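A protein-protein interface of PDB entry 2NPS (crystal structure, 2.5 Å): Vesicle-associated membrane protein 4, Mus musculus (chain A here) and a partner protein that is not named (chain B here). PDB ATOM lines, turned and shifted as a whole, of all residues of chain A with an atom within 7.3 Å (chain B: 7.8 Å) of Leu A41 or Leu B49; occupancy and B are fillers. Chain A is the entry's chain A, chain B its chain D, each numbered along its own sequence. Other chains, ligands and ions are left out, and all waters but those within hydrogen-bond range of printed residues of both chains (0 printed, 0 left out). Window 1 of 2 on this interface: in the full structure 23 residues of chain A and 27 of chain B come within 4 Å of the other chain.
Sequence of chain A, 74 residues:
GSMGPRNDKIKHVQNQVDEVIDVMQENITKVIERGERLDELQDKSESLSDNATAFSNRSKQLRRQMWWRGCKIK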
ATOM      1  N   GLU A  33     -30.600  30.416 -16.601  1.00  0.00           N
ATOM      2  CA  GLU A  33     -30.722  29.007 -16.903  1.00  0.00           C
ATOM      3  C   GLU A  33     -30.265  28.229 -15.677  1.00  0.00           C
ATOM      4  O   GLU A  33     -30.882  27.242 -15.294  1.00  0.00           O
ATOM      5  CB  GLU A  33     -29.862  28.655 -18.127  1.00  0.00           C
ATOM      6  CG  GLU A  33     -30.601  28.782 -19.460  1.00  0.00           C
ATOM      7  CD  GLU A  33     -29.685  28.713 -20.689  1.00  0.00           C
ATOM      8  OE1 GLU A  33     -30.184  28.319 -21.767  1.00  0.00           O
ATOM      9  OE2 GLU A  33     -28.481  29.059 -20.603  1.00  0.00           O
ATOM     10  N   ARG A  34     -29.188  28.687 -15.055  1.00  0.00           N
ATOM     11  CA  ARG A  34     -28.658  28.035 -13.872  1.00  0.00           C
ATOM     12  C   ARG A  34     -29.663  28.064 -12.721  1.00  0.00           C
ATOM     13  O   ARG A  34     -29.802  27.088 -11.983  1.00  0.00           O
ATOM     14  CB  ARG A  34     -27.359  28.714 -13.448  1.00  0.00           C
ATOM     15  CG  ARG A  34     -26.595  27.919 -12.422  1.00  0.00           C
ATOM     16  CD  ARG A  34     -25.261  28.534 -12.049  1.00  0.00           C
ATOM     17  NE  ARG A  34     -25.365  29.304 -10.823  1.00  0.00           N
ATOM     18  CZ  ARG A  34     -24.521  29.210  -9.802  1.00  0.00           C
ATOM     19  NH1 ARG A  34     -24.702  29.961  -8.717  1.00  0.00           N
ATOM     20  NH2 ARG A  34     -23.505  28.371  -9.859  1.00  0.00           N
ATOM     21  N   GLY A  35     -30.360  29.187 -12.569  1.00  0.00           N
ATOM     22  CA  GLY A  35     -31.346  29.300 -11.512  1.00  0.00           C
ATOM     23  C   GLY A  35     -32.450  28.280 -11.709  1.00  0.00           C
ATOM     24  O   GLY A  35     -32.905  27.651 -10.753  1.00  0.00           O
ATOM     25  N   GLU A  36     -32.871  28.108 -12.956  1.00  0.00           N
ATOM     26  CA  GLU A  36     -33.927  27.159 -13.297  1.00  0.00           C
ATOM     27  C   GLU A  36     -33.536  25.716 -13.031  1.00  0.00           C
ATOM     28  O   GLU A  36     -34.365  24.907 -12.603  1.00  0.00           O
ATOM     29  CB  GLU A  36     -34.316  27.297 -14.764  1.00  0.00           C
ATOM     30  CG  GLU A  36     -35.015  28.590 -15.077  1.00  0.00           C
ATOM     31  CD  GLU A  36     -35.677  28.565 -16.433  1.00  0.00           C
ATOM     32  OE1 GLU A  36     -36.248  29.608 -16.850  1.00  0.00           O
ATOM     33  OE2 GLU A  36     -35.634  27.494 -17.074  1.00  0.00           O
ATOM     34  N   ARG A  37     -32.280  25.385 -13.295  1.00  0.00           N
ATOM     35  CA  ARG A  37     -31.824  24.035 -13.053  1.00  0.00           C
ATOM     36  C   ARG A  37     -31.685  23.848 -11.547  1.00  0.00           C
ATOM     37  O   ARG A  37     -31.982  22.779 -11.011  1.00  0.00           O
ATOM     38  CB  ARG A  37     -30.495  23.787 -13.768  1.00  0.00           C
ATOM     39  CG  ARG A  37     -30.465  24.281 -15.217  1.00  0.00           C
ATOM     40  CD  ARG A  37     -31.614  23.729 -16.099  1.00  0.00           C
ATOM     41  NE  ARG A  37     -32.578  24.772 -16.480  1.00  0.00           N
ATOM     42  CZ  ARG A  37     -33.709  24.556 -17.155  1.00  0.00           C
ATOM     43  NH1 ARG A  37     -34.048  23.330 -17.541  1.00  0.00           N
ATOM     44  NH2 ARG A  37     -34.505  25.571 -17.445  1.00  0.00           N
ATOM     45  N   LEU A  38     -31.244  24.889 -10.849  1.00  0.00           N
ATOM     46  CA  LEU A  38     -31.126  24.775  -9.402  1.00  0.00           C
ATOM     47  C   LEU A  38     -32.517  24.567  -8.828  1.00  0.00           C
ATOM     48  O   LEU A  38     -32.696  23.806  -7.886  1.00  0.00           O
ATOM     49  CB  LEU A  38     -30.468  26.019  -8.806  1.00  0.00           C
ATOM     50  CG  LEU A  38     -28.938  26.042  -8.918  1.00  0.00           C
ATOM     51  CD1 LEU A  38     -28.414  27.390  -8.471  1.00  0.00           C
ATOM     52  CD2 LEU A  38     -28.326  24.952  -8.074  1.00  0.00           C
ATOM     53  N   ASP A  39     -33.506  25.230  -9.426  1.00  0.00           N
ATOM     54  CA  ASP A  39     -34.889  25.100  -8.993  1.00  0.00           C
ATOM     55  C   ASP A  39     -35.394  23.676  -9.148  1.00  0.00           C
ATOM     56  O   ASP A  39     -36.087  23.166  -8.276  1.00  0.00           O
ATOM     57  CB  ASP A  39     -35.787  26.061  -9.775  1.00  0.00           C
ATOM     58  CG  ASP A  39     -36.208  27.265  -8.949  1.00  0.00           C
ATOM     59  OD1 ASP A  39     -36.166  28.402  -9.467  1.00  0.00           O
ATOM     60  OD2 ASP A  39     -36.592  27.076  -7.778  1.00  0.00           O
ATOM     61  N   GLU A  40     -35.056  23.025 -10.253  1.00  0.00           N
ATOM     62  CA  GLU A  40     -35.482  21.652 -10.461  1.00  0.00           C
ATOM     63  C   GLU A  40     -34.715  20.736  -9.498  1.00  0.00           C
ATOM     64  O   GLU A  40     -35.264  19.763  -8.987  1.00  0.00           O
ATOM     65  CB  GLU A  40     -35.204  21.207 -11.904  1.00  0.00           C
ATOM     66  CG  GLU A  40     -35.879  22.001 -13.017  1.00  0.00           C
ATOM     67  CD  GLU A  40     -35.537  21.454 -14.416  1.00  0.00           C
ATOM     68  OE1 GLU A  40     -35.865  20.280 -14.701  1.00  0.00           O
ATOM     69  OE2 GLU A  40     -34.934  22.188 -15.232  1.00  0.00           O
ATOM     70  N   LEU A  41     -33.441  21.044  -9.271  1.00  0.00           N
ATOM     71  CA  LEU A  41     -32.595  20.248  -8.383  1.00  0.00           C
ATOM     72  C   LEU A  41     -33.124  20.274  -6.964  1.00  0.00           C
ATOM     73  O   LEU A  41     -33.096  19.276  -6.241  1.00  0.00           O
ATOM     74  CB  LEU A  41     -31.160  20.789  -8.389  1.00  0.00           C
ATOM     75  CG  LEU A  41     -30.056  20.147  -9.245  1.00  0.00           C
ATOM     76  CD1 LEU A  41     -30.629  19.398 -10.431  1.00  0.00           C
ATOM     77  CD2 LEU A  41     -29.101  21.233  -9.719  1.00  0.00           C
ATOM     78  N   GLN A  42     -33.607  21.438  -6.566  1.00  0.00           N
ATOM     79  CA  GLN A  42     -34.123  21.614  -5.238  1.00  0.00           C
ATOM     80  C   GLN A  42     -35.439  20.860  -5.084  1.00  0.00           C
ATOM     81  O   GLN A  42     -35.702  20.265  -4.050  1.00  0.00           O
ATOM     82  CB  GLN A  42     -34.266  23.108  -4.973  1.00  0.00           C
ATOM     83  CG  GLN A  42     -34.186  23.482  -3.515  1.00  0.00           C
ATOM     84  CD  GLN A  42     -35.549  23.610  -2.916  1.00  0.00           C
ATOM     85  OE1 GLN A  42     -36.290  24.527  -3.268  1.00  0.00           O
ATOM     86  NE2 GLN A  42     -35.909  22.687  -2.024  1.00  0.00           N
ATOM     87  N   ASP A  43     -36.251  20.846  -6.132  1.00  0.00           N
ATOM     88  CA  ASP A  43     -37.504  20.118  -6.076  1.00  0.00           C
ATOM     89  C   ASP A  43     -37.268  18.612  -6.004  1.00  0.00           C
ATOM     90  O   ASP A  43     -37.919  17.923  -5.229  1.00  0.00           O
ATOM     91  CB  ASP A  43     -38.378  20.467  -7.277  1.00  0.00           C
ATOM     92  CG  ASP A  43     -39.062  21.827  -7.122  1.00  0.00           C
ATOM     93  OD1 ASP A  43     -40.262  21.952  -7.478  1.00  0.00           O
ATOM     94  OD2 ASP A  43     -38.408  22.784  -6.642  1.00  0.00           O
ATOM     95  N   LYS A  44     -36.324  18.100  -6.791  1.00  0.00           N
ATOM     96  CA  LYS A  44     -36.028  16.674  -6.775  1.00  0.00           C
ATOM     97  C   LYS A  44     -35.356  16.226  -5.490  1.00  0.00           C
ATOM     98  O   LYS A  44     -35.746  15.208  -4.929  1.00  0.00           O
ATOM     99  CB  LYS A  44     -35.142  16.285  -7.947  1.00  0.00           C
ATOM    100  CG  LYS A  44     -35.761  16.455  -9.315  1.00  0.00           C
ATOM    101  CD  LYS A  44     -34.723  16.084 -10.374  1.00  0.00           C
ATOM    102  CE  LYS A  44     -35.243  16.221 -11.788  1.00  0.00           C
ATOM    103  NZ  LYS A  44     -34.192  15.774 -12.738  1.00  0.00           N
ATOM    104  N   SER A  45     -34.355  16.966  -5.013  1.00  0.00           N
ATOM    105  CA  SER A  45     -33.682  16.570  -3.772  1.00  0.00           C
ATOM    106  C   SER A  45     -34.674  16.649  -2.617  1.00  0.00           C
ATOM    107  O   SER A  45     -34.471  16.092  -1.543  1.00  0.00           O
ATOM    108  CB  SER A  45     -32.470  17.456  -3.488  1.00  0.00           C
ATOM    109  OG  SER A  45     -32.861  18.779  -3.221  1.00  0.00           O
ATOM    110  N   GLU A  46     -35.774  17.327  -2.885  1.00  0.00           N
ATOM    111  CA  GLU A  46     -36.856  17.511  -1.952  1.00  0.00           C
ATOM    112  C   GLU A  46     -37.716  16.260  -1.851  1.00  0.00           C
ATOM    113  O   GLU A  46     -38.096  15.846  -0.760  1.00  0.00           O
ATOM    114  CB  GLU A  46     -37.691  18.634  -2.461  1.00  0.00           C
ATOM    115  CG  GLU A  46     -38.325  19.474  -1.444  1.00  0.00           C
ATOM    116  CD  GLU A  46     -39.209  20.452  -2.113  1.00  0.00           C
ATOM    117  OE1 GLU A  46     -40.244  20.014  -2.668  1.00  0.00           O
ATOM    118  OE2 GLU A  46     -38.858  21.646  -2.109  1.00  0.00           O
ATOM    119  N   SER A  47     -38.055  15.676  -2.998  1.00  0.00           N
ATOM    120  CA  SER A  47     -38.838  14.445  -3.021  1.00  0.00           C
ATOM    121  C   SER A  47     -37.996  13.318  -2.459  1.00  0.00           C
ATOM    122  O   SER A  47     -38.499  12.427  -1.789  1.00  0.00           O
ATOM    123  CB  SER A  47     -39.237  14.079  -4.443  1.00  0.00           C
ATOM    124  OG  SER A  47     -39.982  15.122  -5.024  1.00  0.00           O
ATOM    125  N   LEU B  42     -19.675  29.108 -15.891  1.00  0.00           N
ATOM    126  CA  LEU B  42     -21.117  28.917 -15.866  1.00  0.00           C
ATOM    127  C   LEU B  42     -21.514  27.777 -16.790  1.00  0.00           C
ATOM    128  O   LEU B  42     -22.422  27.010 -16.489  1.00  0.00           O
ATOM    129  CB  LEU B  42     -21.836  30.203 -16.275  1.00  0.00           C
ATOM    130  CG  LEU B  42     -21.840  31.315 -15.225  1.00  0.00           C
ATOM    131  CD1 LEU B  42     -22.362  32.618 -15.816  1.00  0.00           C
ATOM    132  CD2 LEU B  42     -22.694  30.885 -14.052  1.00  0.00           C
ATOM    133  N   GLU B  43     -20.830  27.661 -17.921  1.00  0.00           N
ATOM    134  CA  GLU B  43     -21.148  26.598 -18.859  1.00  0.00           C
ATOM    135  C   GLU B  43     -20.731  25.251 -18.284  1.00  0.00           C
ATOM    136  O   GLU B  43     -21.416  24.251 -18.464  1.00  0.00           O
ATOM    137  CB  GLU B  43     -20.459  26.854 -20.196  1.00  0.00           C
ATOM    138  CG  GLU B  43     -20.937  25.935 -21.299  1.00  0.00           C
ATOM    139  CD  GLU B  43     -22.448  25.784 -21.326  1.00  0.00           C
ATOM    140  N   GLU B  44     -19.613  25.251 -17.565  1.00  0.00           N
ATOM    141  CA  GLU B  44     -19.087  24.058 -16.913  1.00  0.00           C
ATOM    142  C   GLU B  44     -19.986  23.563 -15.793  1.00  0.00           C
ATOM    143  O   GLU B  44     -20.119  22.357 -15.564  1.00  0.00           O
ATOM    144  CB  GLU B  44     -17.723  24.336 -16.319  1.00  0.00           C
ATOM    145  CG  GLU B  44     -16.598  24.235 -17.297  1.00  0.00           C
ATOM    146  CD  GLU B  44     -15.273  24.162 -16.587  1.00  0.00           C
ATOM    147  OE1 GLU B  44     -14.231  24.049 -17.269  1.00  0.00           O
ATOM    148  OE2 GLU B  44     -15.290  24.216 -15.335  1.00  0.00           O
ATOM    149  N   GLN B  45     -20.585  24.499 -15.070  1.00  0.00           N
ATOM    150  CA  GLN B  45     -21.479  24.136 -13.994  1.00  0.00           C
ATOM    151  C   GLN B  45     -22.803  23.673 -14.577  1.00  0.00           C
ATOM    152  O   GLN B  45     -23.457  22.798 -14.031  1.00  0.00           O
ATOM    153  CB  GLN B  45     -21.654  25.315 -13.051  1.00  0.00           C
ATOM    154  CG  GLN B  45     -20.471  25.468 -12.119  1.00  0.00           C
ATOM    155  CD  GLN B  45     -20.634  26.594 -11.128  1.00  0.00           C
ATOM    156  OE1 GLN B  45     -21.746  26.934 -10.739  1.00  0.00           O
ATOM    157  NE2 GLN B  45     -19.520  27.166 -10.692  1.00  0.00           N
ATOM    158  N   ALA B  46     -23.177  24.235 -15.717  1.00  0.00           N
ATOM    159  CA  ALA B  46     -24.402  23.816 -16.374  1.00  0.00           C
ATOM    160  C   ALA B  46     -24.303  22.312 -16.642  1.00  0.00           C
ATOM    161  O   ALA B  46     -25.237  21.555 -16.397  1.00  0.00           O
ATOM    162  CB  ALA B  46     -24.587  24.583 -17.669  1.00  0.00           C
ATOM    163  N   VAL B  47     -23.156  21.876 -17.145  1.00  0.00           N
ATOM    164  CA  VAL B  47     -22.961  20.460 -17.396  1.00  0.00           C
ATOM    165  C   VAL B  47     -23.033  19.742 -16.064  1.00  0.00           C
ATOM    166  O   VAL B  47     -23.799  18.806 -15.893  1.00  0.00           O
ATOM    167  CB  VAL B  47     -21.599  20.193 -18.067  1.00  0.00           C
ATOM    168  CG1 VAL B  47     -21.133  18.779 -17.775  1.00  0.00           C
ATOM    169  CG2 VAL B  47     -21.718  20.392 -19.563  1.00  0.00           C
ATOM    170  N   MET B  48     -22.247  20.213 -15.112  1.00  0.00           N
ATOM    171  CA  MET B  48     -22.192  19.618 -13.788  1.00  0.00           C
ATOM    172  C   MET B  48     -23.562  19.540 -13.104  1.00  0.00           C
ATOM    173  O   MET B  48     -23.822  18.618 -12.339  1.00  0.00           O
ATOM    174  CB  MET B  48     -21.213  20.426 -12.936  1.00  0.00           C
ATOM    175  CG  MET B  48     -20.662  19.730 -11.716  1.00  0.00           C
ATOM    176  SD  MET B  48     -19.704  20.890 -10.713  1.00  0.00           S
ATOM    177  CE  MET B  48     -18.371  21.242 -11.809  1.00  0.00           C
ATOM    178  N   LEU B  49     -24.447  20.487 -13.393  1.00  0.00           N
ATOM    179  CA  LEU B  49     -25.776  20.485 -12.774  1.00  0.00           C
ATOM    180  C   LEU B  49     -26.736  19.519 -13.441  1.00  0.00           C
ATOM    181  O   LEU B  49     -27.661  18.989 -12.802  1.00  0.00           O
ATOM    182  CB  LEU B  49     -26.384  21.885 -12.802  1.00  0.00           C
ATOM    183  CG  LEU B  49     -25.630  22.950 -12.012  1.00  0.00           C
ATOM    184  CD1 LEU B  49     -26.193  24.305 -12.344  1.00  0.00           C
ATOM    185  CD2 LEU B  49     -25.705  22.665 -10.521  1.00  0.00           C
ATOM    186  N   GLU B  50     -26.531  19.302 -14.733  1.00  0.00           N
ATOM    187  CA  GLU B  50     -27.392  18.389 -15.434  1.00  0.00           C
ATOM    188  C   GLU B  50     -26.982  16.994 -15.006  1.00  0.00           C
ATOM    189  O   GLU B  50     -27.802  16.085 -14.929  1.00  0.00           O
ATOM    190  CB  GLU B  50     -27.260  18.552 -16.936  1.00  0.00           C
ATOM    191  CG  GLU B  50     -28.428  17.917 -17.629  1.00  0.00           C
ATOM    192  CD  GLU B  50     -28.140  17.540 -19.050  1.00  0.00           C
ATOM    193  OE1 GLU B  50     -28.089  18.453 -19.896  1.00  0.00           O
ATOM    194  OE2 GLU B  50     -27.958  16.330 -19.309  1.00  0.00           O
ATOM    195  N   ASP B  51     -25.701  16.843 -14.703  1.00  0.00           N
ATOM    196  CA  ASP B  51     -25.177  15.564 -14.243  1.00  0.00           C
ATOM    197  C   ASP B  51     -25.775  15.271 -12.874  1.00  0.00           C
ATOM    198  O   ASP B  51     -26.303  14.182 -12.641  1.00  0.00           O
ATOM    199  CB  ASP B  51     -23.640  15.593 -14.148  1.00  0.00           C
ATOM    200  CG  ASP B  51     -22.954  15.482 -15.522  1.00  0.00           C
ATOM    201  OD1 ASP B  51     -21.700  15.522 -15.587  1.00  0.00           O
ATOM    202  OD2 ASP B  51     -23.662  15.348 -16.549  1.00  0.00           O
ATOM    203  N   PHE B  52     -25.701  16.257 -11.981  1.00  0.00           N
ATOM    204  CA  PHE B  52     -26.259  16.148 -10.630  1.00  0.00           C
ATOM    205  C   PHE B  52     -27.756  15.831 -10.745  1.00  0.00           C
ATOM    206  O   PHE B  52     -28.298  15.004 -10.022  1.00  0.00           O
ATOM    207  CB  PHE B  52     -26.043  17.469  -9.873  1.00  0.00           C
ATOM    208  CG  PHE B  52     -26.370  17.398  -8.404  1.00  0.00           C
ATOM    209  CD1 PHE B  52     -26.389  18.551  -7.637  1.00  0.00           C
ATOM    210  CD2 PHE B  52     -26.646  16.189  -7.785  1.00  0.00           C
ATOM    211  CE1 PHE B  52     -26.674  18.505  -6.270  1.00  0.00           C
ATOM    212  CE2 PHE B  52     -26.933  16.130  -6.421  1.00  0.00           C
ATOM    213  CZ  PHE B  52     -26.947  17.294  -5.658  1.00  0.00           C
ATOM    214  N   SER B  53     -28.421  16.491 -11.670  1.00  0.00           N
ATOM    215  CA  SER B  53     -29.818  16.221 -11.857  1.00  0.00           C
ATOM    216  C   SER B  53     -30.057  14.756 -12.201  1.00  0.00           C
ATOM    217  O   SER B  53     -30.967  14.140 -11.663  1.00  0.00           O
ATOM    218  CB  SER B  53     -30.377  17.092 -12.965  1.00  0.00           C
ATOM    219  OG  SER B  53     -31.719  16.731 -13.194  1.00  0.00           O
ATOM    220  N   HIS B  54     -29.243  14.190 -13.090  1.00  0.00           N
ATOM    221  CA  HIS B  54     -29.439  12.795 -13.484  1.00  0.00           C
ATOM    222  C   HIS B  54     -29.121  11.787 -12.402  1.00  0.00           C
ATOM    223  O   HIS B  54     -29.772  10.749 -12.291  1.00  0.00           O
ATOM    224  CB  HIS B  54     -28.650  12.481 -14.758  1.00  0.00           C
ATOM    225  CG  HIS B  54     -29.251  13.105 -15.980  1.00  0.00           C
ATOM    226  ND1 HIS B  54     -30.552  12.859 -16.365  1.00  0.00           N
ATOM    227  CD2 HIS B  54     -28.784  14.057 -16.824  1.00  0.00           C
ATOM    228  CE1 HIS B  54     -30.865  13.639 -17.385  1.00  0.00           C
ATOM    229  NE2 HIS B  54     -29.810  14.376 -17.682  1.00  0.00           N
ATOM    230  N   GLU B  55     -28.130  12.102 -11.589  1.00  0.00           N
ATOM    231  CA  GLU B  55     -27.770  11.227 -10.504  1.00  0.00           C
ATOM    232  C   GLU B  55     -28.922  11.245  -9.494  1.00  0.00           C
ATOM    233  O   GLU B  55     -29.277  10.209  -8.930  1.00  0.00           O
ATOM    234  CB  GLU B  55     -26.480  11.717  -9.886  1.00  0.00           C
ATOM    235  CG  GLU B  55     -25.426  11.953 -10.942  1.00  0.00           C
ATOM    236  CD  GLU B  55     -24.203  12.638 -10.399  1.00  0.00           C
ATOM    237  OE1 GLU B  55     -23.332  13.018 -11.215  1.00  0.00           O
ATOM    238  OE2 GLU B  55     -24.118  12.792  -9.157  1.00  0.00           O
ATOM    239  N   LEU B  56     -29.517  12.421  -9.278  1.00  0.00           N
ATOM    240  CA  LEU B  56     -30.645  12.553  -8.371  1.00  0.00           C
ATOM    241  C   LEU B  56     -31.746  11.640  -8.851  1.00  0.00           C
ATOM    242  O   LEU B  56     -32.272  10.865  -8.076  1.00  0.00           O
ATOM    243  CB  LEU B  56     -31.166  13.992  -8.345  1.00  0.00           C
ATOM    244  CG  LEU B  56     -30.632  15.002  -7.328  1.00  0.00           C
ATOM    245  CD1 LEU B  56     -31.291  16.354  -7.526  1.00  0.00           C
ATOM    246  CD2 LEU B  56     -30.921  14.509  -5.926  1.00  0.00           C
ATOM    247  N   GLU B  57     -32.099  11.743 -10.130  1.00  0.00           N
ATOM    248  CA  GLU B  57     -33.144  10.900 -10.735  1.00  0.00           C
ATOM    249  C   GLU B  57     -32.860   9.412 -10.540  1.00  0.00           C
ATOM    250  O   GLU B  57     -33.760   8.608 -10.296  1.00  0.00           O
ATOM    251  CB  GLU B  57     -33.258  11.189 -12.230  1.00  0.00           C
ATOM    252  CG  GLU B  57     -34.247  12.300 -12.591  1.00  0.00           C
ATOM    253  CD  GLU B  57     -34.248  12.630 -14.087  1.00  0.00           C
ATOM    254  OE1 GLU B  57     -34.436  11.707 -14.916  1.00  0.00           O
ATOM    255  OE2 GLU B  57     -34.060  13.815 -14.434  1.00  0.00           O
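The guanidinium group of Arg A34 lies within hydrogen-bond range of the side-chain amide oxygen of Gln B45, at 2.4 Å. The side-chain carboxylate of Glu B57 is in salt-bridge range of the side-chain amino group of Lys A44 (2.6 Å). The side-chain amino group of Lys A44 lies within hydrogen-bond range of the side-chain hydroxyl of Ser B53, at 2.7 Å.
The backbone carbonyl oxygen (O) of Leu A41 lies within hydrogen-bond range of the side-chain hydroxyl (OG) of Ser A45 (3.1 Å).
Leu B49 touches Arg A34 (CD1 to CG, 3.6 Å). CD2 of Leu A41 touches CD2 of Leu B49 (3.8 Å). CD1 of Leu A41 touches CB of Ser B53, at 3.4 Å. Leu A41 touches Leu B56. CB of Lys A44 touches CD1 of Leu B56, 3.9 Å away.
Of the printed residues of chain A, Glu B57 touches Lys A44 (2.6 Å). Of the printed residues of chain A, Leu B56 touches Leu A41 and Lys A44. Of the printed residues of chain A, Gln B45 touches Arg A34. Of the printed residues of chain B, Lys A44 touches Ser B53, Leu B56 and Glu B57. Asp A39 touches none of the printed residues of chain B. Glu B44 touches none of the printed residues of chain A. The nearest residue of chain B that does not touch Leu A41 is Phe B52 (4.3 Å). The nearest residue of chain A that does not touch Leu B49 is Leu A38 (4.3 Å). The nearest printed residue of chain A that does not touch Gln B45 is Leu A38 (7.1 Å).
Printed residues of chain B that touch a printed residue of chain A: Gln B45, Leu B49, Ser B53, Leu B56 and Glu B57. Hydrophobic or aromatic side chains of chain B that line the printed part of chain A: Leu B49 and Leu B56. Along chain B the printed residues that touch a printed residue of chain A span positions 45 to 57. Of the 15 printed residues of chain A, 3 touch a printed residue of chain B. Printed residues of chain A that touch a printed residue of chain B: Arg A34, Leu A41 and Lys A44. Hydrophobic or aromatic side chains of chain A within 4 Å of the printed part of chain B: Leu A41.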
